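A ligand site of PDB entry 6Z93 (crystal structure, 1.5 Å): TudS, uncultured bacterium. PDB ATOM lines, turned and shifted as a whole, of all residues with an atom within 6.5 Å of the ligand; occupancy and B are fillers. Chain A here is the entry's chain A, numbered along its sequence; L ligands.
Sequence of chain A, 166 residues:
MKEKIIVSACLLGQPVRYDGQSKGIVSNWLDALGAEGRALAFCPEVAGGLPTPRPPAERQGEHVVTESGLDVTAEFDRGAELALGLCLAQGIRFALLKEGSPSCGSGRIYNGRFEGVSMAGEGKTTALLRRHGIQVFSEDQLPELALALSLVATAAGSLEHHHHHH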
ATOM      1  N   VAL A   7      36.870  17.688 -10.429  1.00  0.00           N
ATOM      2  CA  VAL A   7      35.590  17.679  -9.724  1.00  0.00           C
ATOM      3  C   VAL A   7      34.709  16.590 -10.277  1.00  0.00           C
ATOM      4  O   VAL A   7      34.597  16.503 -11.491  1.00  0.00           O
ATOM      5  CB  VAL A   7      34.860  19.042  -9.904  1.00  0.00           C
ATOM      6  CG1 VAL A   7      33.553  19.075  -9.108  1.00  0.00           C
ATOM      7  CG2 VAL A   7      35.754  20.219  -9.526  1.00  0.00           C
ATOM      8  N   SER A   8      33.987  15.811  -9.428  1.00  0.00           N
ATOM      9  CA  SER A   8      32.994  14.824  -9.913  1.00  0.00           C
ATOM     10  C   SER A   8      32.007  15.526 -10.846  1.00  0.00           C
ATOM     11  O   SER A   8      31.469  16.565 -10.469  1.00  0.00           O
ATOM     12  CB  SER A   8      32.199  14.254  -8.742  1.00  0.00           C
ATOM     13  OG  SER A   8      32.974  13.347  -7.985  1.00  0.00           O
ATOM     14  N   ALA A   9      31.876  15.032 -12.089  1.00  0.00           N
ATOM     15  CA  ALA A   9      31.025  15.686 -13.089  1.00  0.00           C
ATOM     16  C   ALA A   9      29.601  15.914 -12.642  1.00  0.00           C
ATOM     17  O   ALA A   9      29.017  16.953 -12.985  1.00  0.00           O
ATOM     18  CB  ALA A   9      31.068  14.909 -14.408  1.00  0.00           C
ATOM     19  N   CYS A  10      29.047  15.017 -11.803  1.00  0.00           N
ATOM     20  CA  CYS A  10      27.691  15.168 -11.279  1.00  0.00           C
ATOM     21  C   CYS A  10      27.584  16.403 -10.359  1.00  0.00           C
ATOM     22  O   CYS A  10      26.535  17.058 -10.342  1.00  0.00           O
ATOM     23  CB  CYS A  10      27.224  13.897 -10.568  1.00  0.00           C
ATOM     24  SG  CYS A  10      28.254  13.413  -9.147  1.00  0.00           S
ATOM     25  N   LEU A  11      28.651  16.757  -9.618  1.00  0.00           N
ATOM     26  CA  LEU A  11      28.626  17.957  -8.750  1.00  0.00           C
ATOM     27  C   LEU A  11      28.555  19.242  -9.550  1.00  0.00           C
ATOM     28  O   LEU A  11      28.128  20.270  -9.017  1.00  0.00           O
ATOM     29  CB  LEU A  11      29.837  18.000  -7.841  1.00  0.00           C
ATOM     30  CG  LEU A  11      29.892  16.889  -6.774  1.00  0.00           C
ATOM     31  CD1 LEU A  11      31.210  16.965  -5.987  1.00  0.00           C
ATOM     32  CD2 LEU A  11      28.708  16.982  -5.807  1.00  0.00           C
ATOM     33  N   GLN A  14      26.229  17.751 -14.369  1.00  0.00           N
ATOM     34  CA  GLN A  14      26.165  16.853 -15.513  1.00  0.00           C
ATOM     35  C   GLN A  14      25.333  15.636 -15.187  1.00  0.00           C
ATOM     36  O   GLN A  14      25.428  15.087 -14.090  1.00  0.00           O
ATOM     37  CB  GLN A  14      27.557  16.486 -15.971  1.00  0.00           C
ATOM     38  CG  GLN A  14      28.375  17.732 -16.333  1.00  0.00           C
ATOM     39  CD  GLN A  14      29.624  17.405 -17.076  1.00  0.00           C
ATOM     40  OE1 GLN A  14      29.781  16.311 -17.615  1.00  0.00           O
ATOM     41  NE2 GLN A  14      30.530  18.350 -17.140  1.00  0.00           N
ATOM     42  N   VAL A  16      25.256  12.474 -15.298  1.00  0.00           N
ATOM     43  CA  VAL A  16      26.024  11.237 -15.461  1.00  0.00           C
ATOM     44  C   VAL A  16      25.830  10.235 -14.322  1.00  0.00           C
ATOM     45  O   VAL A  16      26.486   9.187 -14.354  1.00  0.00           O
ATOM     46  CB  VAL A  16      27.538  11.551 -15.615  1.00  0.00           C
ATOM     47  CG1 VAL A  16      27.835  12.196 -16.970  1.00  0.00           C
ATOM     48  CG2 VAL A  16      28.036  12.431 -14.462  1.00  0.00           C
ATOM     49  N   ARG A  17      24.943  10.502 -13.333  1.00  0.00           N
ATOM     50  CA  ARG A  17      24.721   9.568 -12.223  1.00  0.00           C
ATOM     51  C   ARG A  17      24.131   8.259 -12.732  1.00  0.00           C
ATOM     52  O   ARG A  17      23.611   8.231 -13.846  1.00  0.00           O
ATOM     53  CB  ARG A  17      23.816  10.190 -11.147  1.00  0.00           C
ATOM     54  CG  ARG A  17      24.470  11.331 -10.382  1.00  0.00           C
ATOM     55  CD  ARG A  17      25.322  10.803  -9.234  1.00  0.00           C
ATOM     56  NE  ARG A  17      24.490  10.264  -8.160  1.00  0.00           N
ATOM     57  CZ  ARG A  17      24.957   9.832  -7.000  1.00  0.00           C
ATOM     58  NH1 ARG A  17      26.256   9.878  -6.739  1.00  0.00           N
ATOM     59  NH2 ARG A  17      24.119   9.355  -6.070  1.00  0.00           N
ATOM     60  N   TYR A  18      24.148   7.184 -11.914  1.00  0.00           N
ATOM     61  CA  TYR A  18      23.602   5.897 -12.357  1.00  0.00           C
ATOM     62  C   TYR A  18      22.135   6.010 -12.836  1.00  0.00           C
ATOM     63  O   TYR A  18      21.711   5.206 -13.652  1.00  0.00           O
ATOM     64  CB  TYR A  18      23.721   4.822 -11.262  1.00  0.00           C
ATOM     65  CG  TYR A  18      22.676   4.959 -10.182  1.00  0.00           C
ATOM     66  CD1 TYR A  18      22.736   5.988  -9.254  1.00  0.00           C
ATOM     67  CD2 TYR A  18      21.591   4.106 -10.131  1.00  0.00           C
ATOM     68  CE1 TYR A  18      21.749   6.146  -8.286  1.00  0.00           C
ATOM     69  CE2 TYR A  18      20.603   4.242  -9.158  1.00  0.00           C
ATOM     70  CZ  TYR A  18      20.680   5.264  -8.243  1.00  0.00           C
ATOM     71  OH  TYR A  18      19.713   5.380  -7.278  1.00  0.00           O
ATOM     72  N   GLN A  21      20.491  11.260 -13.184  1.00  0.00           N
ATOM     73  CA  GLN A  21      20.365  12.521 -12.455  1.00  0.00           C
ATOM     74  C   GLN A  21      21.719  13.239 -12.365  1.00  0.00           C
ATOM     75  O   GLN A  21      22.752  12.724 -12.791  1.00  0.00           O
ATOM     76  CB  GLN A  21      19.860  12.263 -11.030  1.00  0.00           C
ATOM     77  CG  GLN A  21      18.390  11.842 -10.922  1.00  0.00           C
ATOM     78  CD  GLN A  21      17.956  12.167  -9.523  1.00  0.00           C
ATOM     79  OE1 GLN A  21      17.280  13.174  -9.273  1.00  0.00           O
ATOM     80  NE2 GLN A  21      18.347  11.336  -8.553  1.00  0.00           N
ATOM     81  N   LYS A  23      24.004  15.993  -9.496  1.00  0.00           N
ATOM     82  CA  LYS A  23      24.092  16.346  -8.072  1.00  0.00           C
ATOM     83  C   LYS A  23      24.661  17.755  -7.991  1.00  0.00           C
ATOM     84  O   LYS A  23      25.621  18.003  -7.240  1.00  0.00           O
ATOM     85  CB  LYS A  23      24.992  15.329  -7.351  1.00  0.00           C
ATOM     86  CG  LYS A  23      24.370  13.938  -7.257  1.00  0.00           C
ATOM     87  CD  LYS A  23      23.103  13.940  -6.385  1.00  0.00           C
ATOM     88  CE  LYS A  23      22.536  12.564  -6.148  1.00  0.00           C
ATOM     89  NZ  LYS A  23      21.242  12.615  -5.418  1.00  0.00           N
ATOM     90  N   PHE A  42      35.004  15.479 -14.263  1.00  0.00           N
ATOM     91  CA  PHE A  42      35.437  14.111 -14.558  1.00  0.00           C
ATOM     92  C   PHE A  42      34.492  13.143 -13.896  1.00  0.00           C
ATOM     93  O   PHE A  42      34.156  13.332 -12.728  1.00  0.00           O
ATOM     94  CB  PHE A  42      36.869  13.881 -14.049  1.00  0.00           C
ATOM     95  CG  PHE A  42      37.401  12.528 -14.445  1.00  0.00           C
ATOM     96  CD1 PHE A  42      37.376  11.458 -13.558  1.00  0.00           C
ATOM     97  CD2 PHE A  42      37.871  12.304 -15.728  1.00  0.00           C
ATOM     98  CE1 PHE A  42      37.828  10.205 -13.936  1.00  0.00           C
ATOM     99  CE2 PHE A  42      38.347  11.040 -16.092  1.00  0.00           C
ATOM    100  CZ  PHE A  42      38.314  10.007 -15.206  1.00  0.00           C
ATOM    101  N   CYS A  43      34.074  12.104 -14.634  1.00  0.00           N
ATOM    102  CA  CYS A  43      33.213  11.066 -14.015  1.00  0.00           C
ATOM    103  C   CYS A  43      33.943   9.749 -14.216  1.00  0.00           C
ATOM    104  O   CYS A  43      33.991   9.237 -15.333  1.00  0.00           O
ATOM    105  CB  CYS A  43      31.826  11.016 -14.637  1.00  0.00           C
ATOM    106  SG  CYS A  43      30.843   9.586 -14.093  1.00  0.00           S
ATOM    107  N   PRO A  44      34.502   9.179 -13.139  1.00  0.00           N
ATOM    108  CA  PRO A  44      35.207   7.893 -13.279  1.00  0.00           C
ATOM    109  C   PRO A  44      34.399   6.751 -13.885  1.00  0.00           C
ATOM    110  O   PRO A  44      34.962   5.930 -14.596  1.00  0.00           O
ATOM    111  CB  PRO A  44      35.603   7.560 -11.820  1.00  0.00           C
ATOM    112  CG  PRO A  44      35.613   8.880 -11.098  1.00  0.00           C
ATOM    113  CD  PRO A  44      34.535   9.700 -11.747  1.00  0.00           C
ATOM    114  N   GLU A  45      33.093   6.655 -13.559  1.00  0.00           N
ATOM    115  CA  GLU A  45      32.313   5.531 -14.095  1.00  0.00           C
ATOM    116  C   GLU A  45      32.082   5.660 -15.583  1.00  0.00           C
ATOM    117  O   GLU A  45      32.203   4.654 -16.300  1.00  0.00           O
ATOM    118  CB  GLU A  45      31.035   5.321 -13.301  1.00  0.00           C
ATOM    119  CG  GLU A  45      31.402   4.904 -11.897  1.00  0.00           C
ATOM    120  CD  GLU A  45      30.292   4.874 -10.875  1.00  0.00           C
ATOM    121  OE1 GLU A  45      29.114   4.778 -11.280  1.00  0.00           O
ATOM    122  OE2 GLU A  45      30.612   4.966  -9.663  1.00  0.00           O
ATOM    123  N   VAL A  46      31.758   6.873 -16.065  1.00  0.00           N
ATOM    124  CA  VAL A  46      31.574   7.045 -17.513  1.00  0.00           C
ATOM    125  C   VAL A  46      32.931   6.921 -18.216  1.00  0.00           C
ATOM    126  O   VAL A  46      33.039   6.238 -19.253  1.00  0.00           O
ATOM    127  CB  VAL A  46      30.873   8.377 -17.821  1.00  0.00           C
ATOM    128  CG1 VAL A  46      30.891   8.679 -19.291  1.00  0.00           C
ATOM    129  CG2 VAL A  46      29.427   8.338 -17.295  1.00  0.00           C
ATOM    130  N   ARG A  54      22.864   3.159 -15.449  1.00  0.00           N
ATOM    131  CA  ARG A  54      23.569   1.914 -15.146  1.00  0.00           C
ATOM    132  C   ARG A  54      23.051   1.433 -13.784  1.00  0.00           C
ATOM    133  O   ARG A  54      22.556   2.243 -12.987  1.00  0.00           O
ATOM    134  CB  ARG A  54      25.089   2.131 -15.102  1.00  0.00           C
ATOM    135  CG  ARG A  54      25.530   3.274 -14.187  1.00  0.00           C
ATOM    136  CD  ARG A  54      27.030   3.574 -14.369  1.00  0.00           C
ATOM    137  NE  ARG A  54      27.447   4.731 -13.563  1.00  0.00           N
ATOM    138  CZ  ARG A  54      27.270   6.006 -13.931  1.00  0.00           C
ATOM    139  NH1 ARG A  54      26.689   6.292 -15.099  1.00  0.00           N
ATOM    140  NH2 ARG A  54      27.668   6.986 -13.145  1.00  0.00           N
ATOM    141  N   PHE A  76      35.490   0.422 -12.890  1.00  0.00           N
ATOM    142  CA  PHE A  76      35.756   1.308 -11.750  1.00  0.00           C
ATOM    143  C   PHE A  76      37.272   1.591 -11.653  1.00  0.00           C
ATOM    144  O   PHE A  76      37.677   2.729 -11.418  1.00  0.00           O
ATOM    145  CB  PHE A  76      35.274   0.670 -10.440  1.00  0.00           C
ATOM    146  CG  PHE A  76      33.821   1.015 -10.161  1.00  0.00           C
ATOM    147  CD1 PHE A  76      32.806   0.497 -10.944  1.00  0.00           C
ATOM    148  CD2 PHE A  76      33.499   1.905  -9.158  1.00  0.00           C
ATOM    149  CE1 PHE A  76      31.480   0.875 -10.718  1.00  0.00           C
ATOM    150  CE2 PHE A  76      32.165   2.265  -8.934  1.00  0.00           C
ATOM    151  CZ  PHE A  76      31.165   1.739  -9.706  1.00  0.00           C
ATOM    152  N   LEU A  97      35.150  15.450  -4.805  1.00  0.00           N
ATOM    153  CA  LEU A  97      34.398  14.300  -5.285  1.00  0.00           C
ATOM    154  C   LEU A  97      33.112  14.050  -4.487  1.00  0.00           C
ATOM    155  O   LEU A  97      33.034  14.386  -3.313  1.00  0.00           O
ATOM    156  CB  LEU A  97      35.293  13.045  -5.281  1.00  0.00           C
ATOM    157  CG  LEU A  97      36.633  13.138  -6.017  1.00  0.00           C
ATOM    158  CD1 LEU A  97      37.363  11.759  -6.008  1.00  0.00           C
ATOM    159  CD2 LEU A  97      36.433  13.537  -7.476  1.00  0.00           C
ATOM    160  N   LYS A  98      32.127  13.426  -5.137  1.00  0.00           N
ATOM    161  CA  LYS A  98      30.797  13.170  -4.593  1.00  0.00           C
ATOM    162  C   LYS A  98      30.802  12.156  -3.435  1.00  0.00           C
ATOM    163  O   LYS A  98      31.218  11.010  -3.601  1.00  0.00           O
ATOM    164  CB  LYS A  98      29.848  12.721  -5.725  1.00  0.00           C
ATOM    165  CG  LYS A  98      28.451  12.323  -5.257  1.00  0.00           C
ATOM    166  CD  LYS A  98      27.612  13.551  -4.853  1.00  0.00           C
ATOM    167  CE  LYS A  98      26.385  13.175  -4.041  1.00  0.00           C
ATOM    168  NZ  LYS A  98      26.724  12.814  -2.631  1.00  0.00           N
ATOM    169  N   GLU A  99      30.279  12.560  -2.276  1.00  0.00           N
ATOM    170  CA  GLU A  99      30.234  11.677  -1.104  1.00  0.00           C
ATOM    171  C   GLU A  99      29.318  10.450  -1.309  1.00  0.00           C
ATOM    172  O   GLU A  99      28.345  10.547  -2.049  1.00  0.00           O
ATOM    173  CB  GLU A  99      29.780  12.487   0.122  1.00  0.00           C
ATOM    174  CG  GLU A  99      29.921  11.736   1.438  1.00  0.00           C
ATOM    175  CD  GLU A  99      31.352  11.284   1.727  1.00  0.00           C
ATOM    176  OE1 GLU A  99      31.810  10.288   1.111  1.00  0.00           O
ATOM    177  OE2 GLU A  99      31.996  11.910   2.608  1.00  0.00           O
ATOM    178  N   SER A 101      29.712   7.629  -2.929  1.00  0.00           N
ATOM    179  CA  SER A 101      29.803   6.862  -4.177  1.00  0.00           C
ATOM    180  C   SER A 101      30.856   5.730  -4.090  1.00  0.00           C
ATOM    181  O   SER A 101      31.924   5.925  -3.523  1.00  0.00           O
ATOM    182  CB  SER A 101      30.113   7.823  -5.325  1.00  0.00           C
ATOM    183  OG  SER A 101      30.691   7.206  -6.466  1.00  0.00           O
ATOM    184  N   PRO A 102      30.592   4.587  -4.746  1.00  0.00           N
ATOM    185  CA  PRO A 102      31.609   3.520  -4.796  1.00  0.00           C
ATOM    186  C   PRO A 102      32.862   3.916  -5.574  1.00  0.00           C
ATOM    187  O   PRO A 102      33.874   3.220  -5.486  1.00  0.00           O
ATOM    188  CB  PRO A 102      30.865   2.363  -5.491  1.00  0.00           C
ATOM    189  CG  PRO A 102      29.813   3.035  -6.326  1.00  0.00           C
ATOM    190  CD  PRO A 102      29.380   4.245  -5.534  1.00  0.00           C
ATOM    191  N   SER A 103      32.801   5.042  -6.346  1.00  0.00           N
ATOM    192  CA  SER A 103      33.961   5.620  -7.029  1.00  0.00           C
ATOM    193  C   SER A 103      34.470   6.846  -6.257  1.00  0.00           C
ATOM    194  O   SER A 103      35.662   6.929  -5.981  1.00  0.00           O
ATOM    195  CB  SER A 103      33.580   6.141  -8.415  1.00  0.00           C
ATOM    196  OG  SER A 103      33.394   5.104  -9.352  1.00  0.00           O
ATOM    197  N   CYS A 104      33.580   7.828  -5.991  1.00  0.00           N
ATOM    198  CA  CYS A 104      33.914   9.164  -5.501  1.00  0.00           C
ATOM    199  C   CYS A 104      33.820   9.388  -3.988  1.00  0.00           C
ATOM    200  O   CYS A 104      34.302  10.418  -3.514  1.00  0.00           O
ATOM    201  CB  CYS A 104      33.067  10.171  -6.272  1.00  0.00           C
ATOM    202  SG  CYS A 104      33.410  10.184  -8.058  1.00  0.00           S
ATOM    203  N   GLY A 105      33.203   8.478  -3.239  1.00  0.00           N
ATOM    204  CA  GLY A 105      33.060   8.616  -1.792  1.00  0.00           C
ATOM    205  C   GLY A 105      34.375   8.860  -1.077  1.00  0.00           C
ATOM    206  O   GLY A 105      35.407   8.358  -1.530  1.00  0.00           O
HETATM  207 FE1  LIG L   1      29.011   8.758  -9.886  1.00  0.00          FE
HETATM  208 FE2  LIG L   1      29.268  11.525  -9.883  1.00  0.00          FE
HETATM  209 FE3  LIG L   1      30.425   9.977 -11.900  1.00  0.00          FE
HETATM  210 FE4  LIG L   1      31.443   9.964  -9.310  1.00  0.00          FE
HETATM  211  S1  LIG L   1      31.378  11.751 -10.805  1.00  0.00           S
HETATM  212  S2  LIG L   1      31.118   8.114 -10.660  1.00  0.00           S
HETATM  213  S3  LIG L   1      29.494  10.106  -8.076  1.00  0.00           S
HETATM  214  S4  LIG L   1      28.163  10.251 -11.470  1.00  0.00           S
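A sulfur (S4) of the ligand sits close to the backbone carbonyl oxygen of Val 16 (3.5 Å).
O of Phe 42 sits close to S1 of the ligand, 3.7 Å away.
Merely in contact with the ligand: Lys 98, Ser 103 and Pro 44.
The side-chain sulfur (SG) of Cys 104 binds an iron atom (FE4) of the ligand (2.3 Å).
The guanidinium group (NH1) of Arg 17 lies close to a sulfur (S3) of the ligand, 3.5 Å away.
The guanidinium group of Arg 54 sits close to a sulfur (S4) of the ligand (3.7 Å).
The backbone NH (N) of Ala 9 sits close to a sulfur (S1) of the ligand (3.6 Å).
The side-chain hydroxyl of Ser 8 lies close to a sulfur (S1) of the ligand, at 3.6 Å.
The backbone NH (N) of Glu 45 sits close to a sulfur (S2) of the ligand, 3.8 Å away.
FE3 of the ligand is bound by SG of Cys 43, 2.3 Å away.
A sulfur (S3) of the ligand sits close to the side-chain hydroxyl (OG) of Ser 101 (3.5 Å).
The backbone NH (N) of Arg 17 sits close to a sulfur (S4) of the ligand, 3.7 Å away.
FE2 of the ligand is bound by SG of Cys 10 (2.3 Å).
OE2 of Glu 45 lies within hydrogen-bond range of OG of Ser 103, 2.8 Å away.
OG of Ser 101 is in hydrogen-bond range of N of Ser 103 (3.0 Å).
O of Ala 9 sits at hydrogen-bond distance from N of Gln 14 (3.2 Å).
The backbone NH (N) of Cys 104 sits at hydrogen-bond distance from the side-chain hydroxyl (OG) of Ser 101, 3.0 Å away.
The side-chain sulfur (SG) of Cys 43 lies close to the backbone NH (N) of Glu 45, at 3.7 Å.
OG of Ser 8 is in hydrogen-bond range of N of Lys 98 (3.0 Å).
SG of Cys 104 sits close to OG of Ser 8 (3.2 Å).
O of Val 7 lies within hydrogen-bond range of N of Phe 42.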
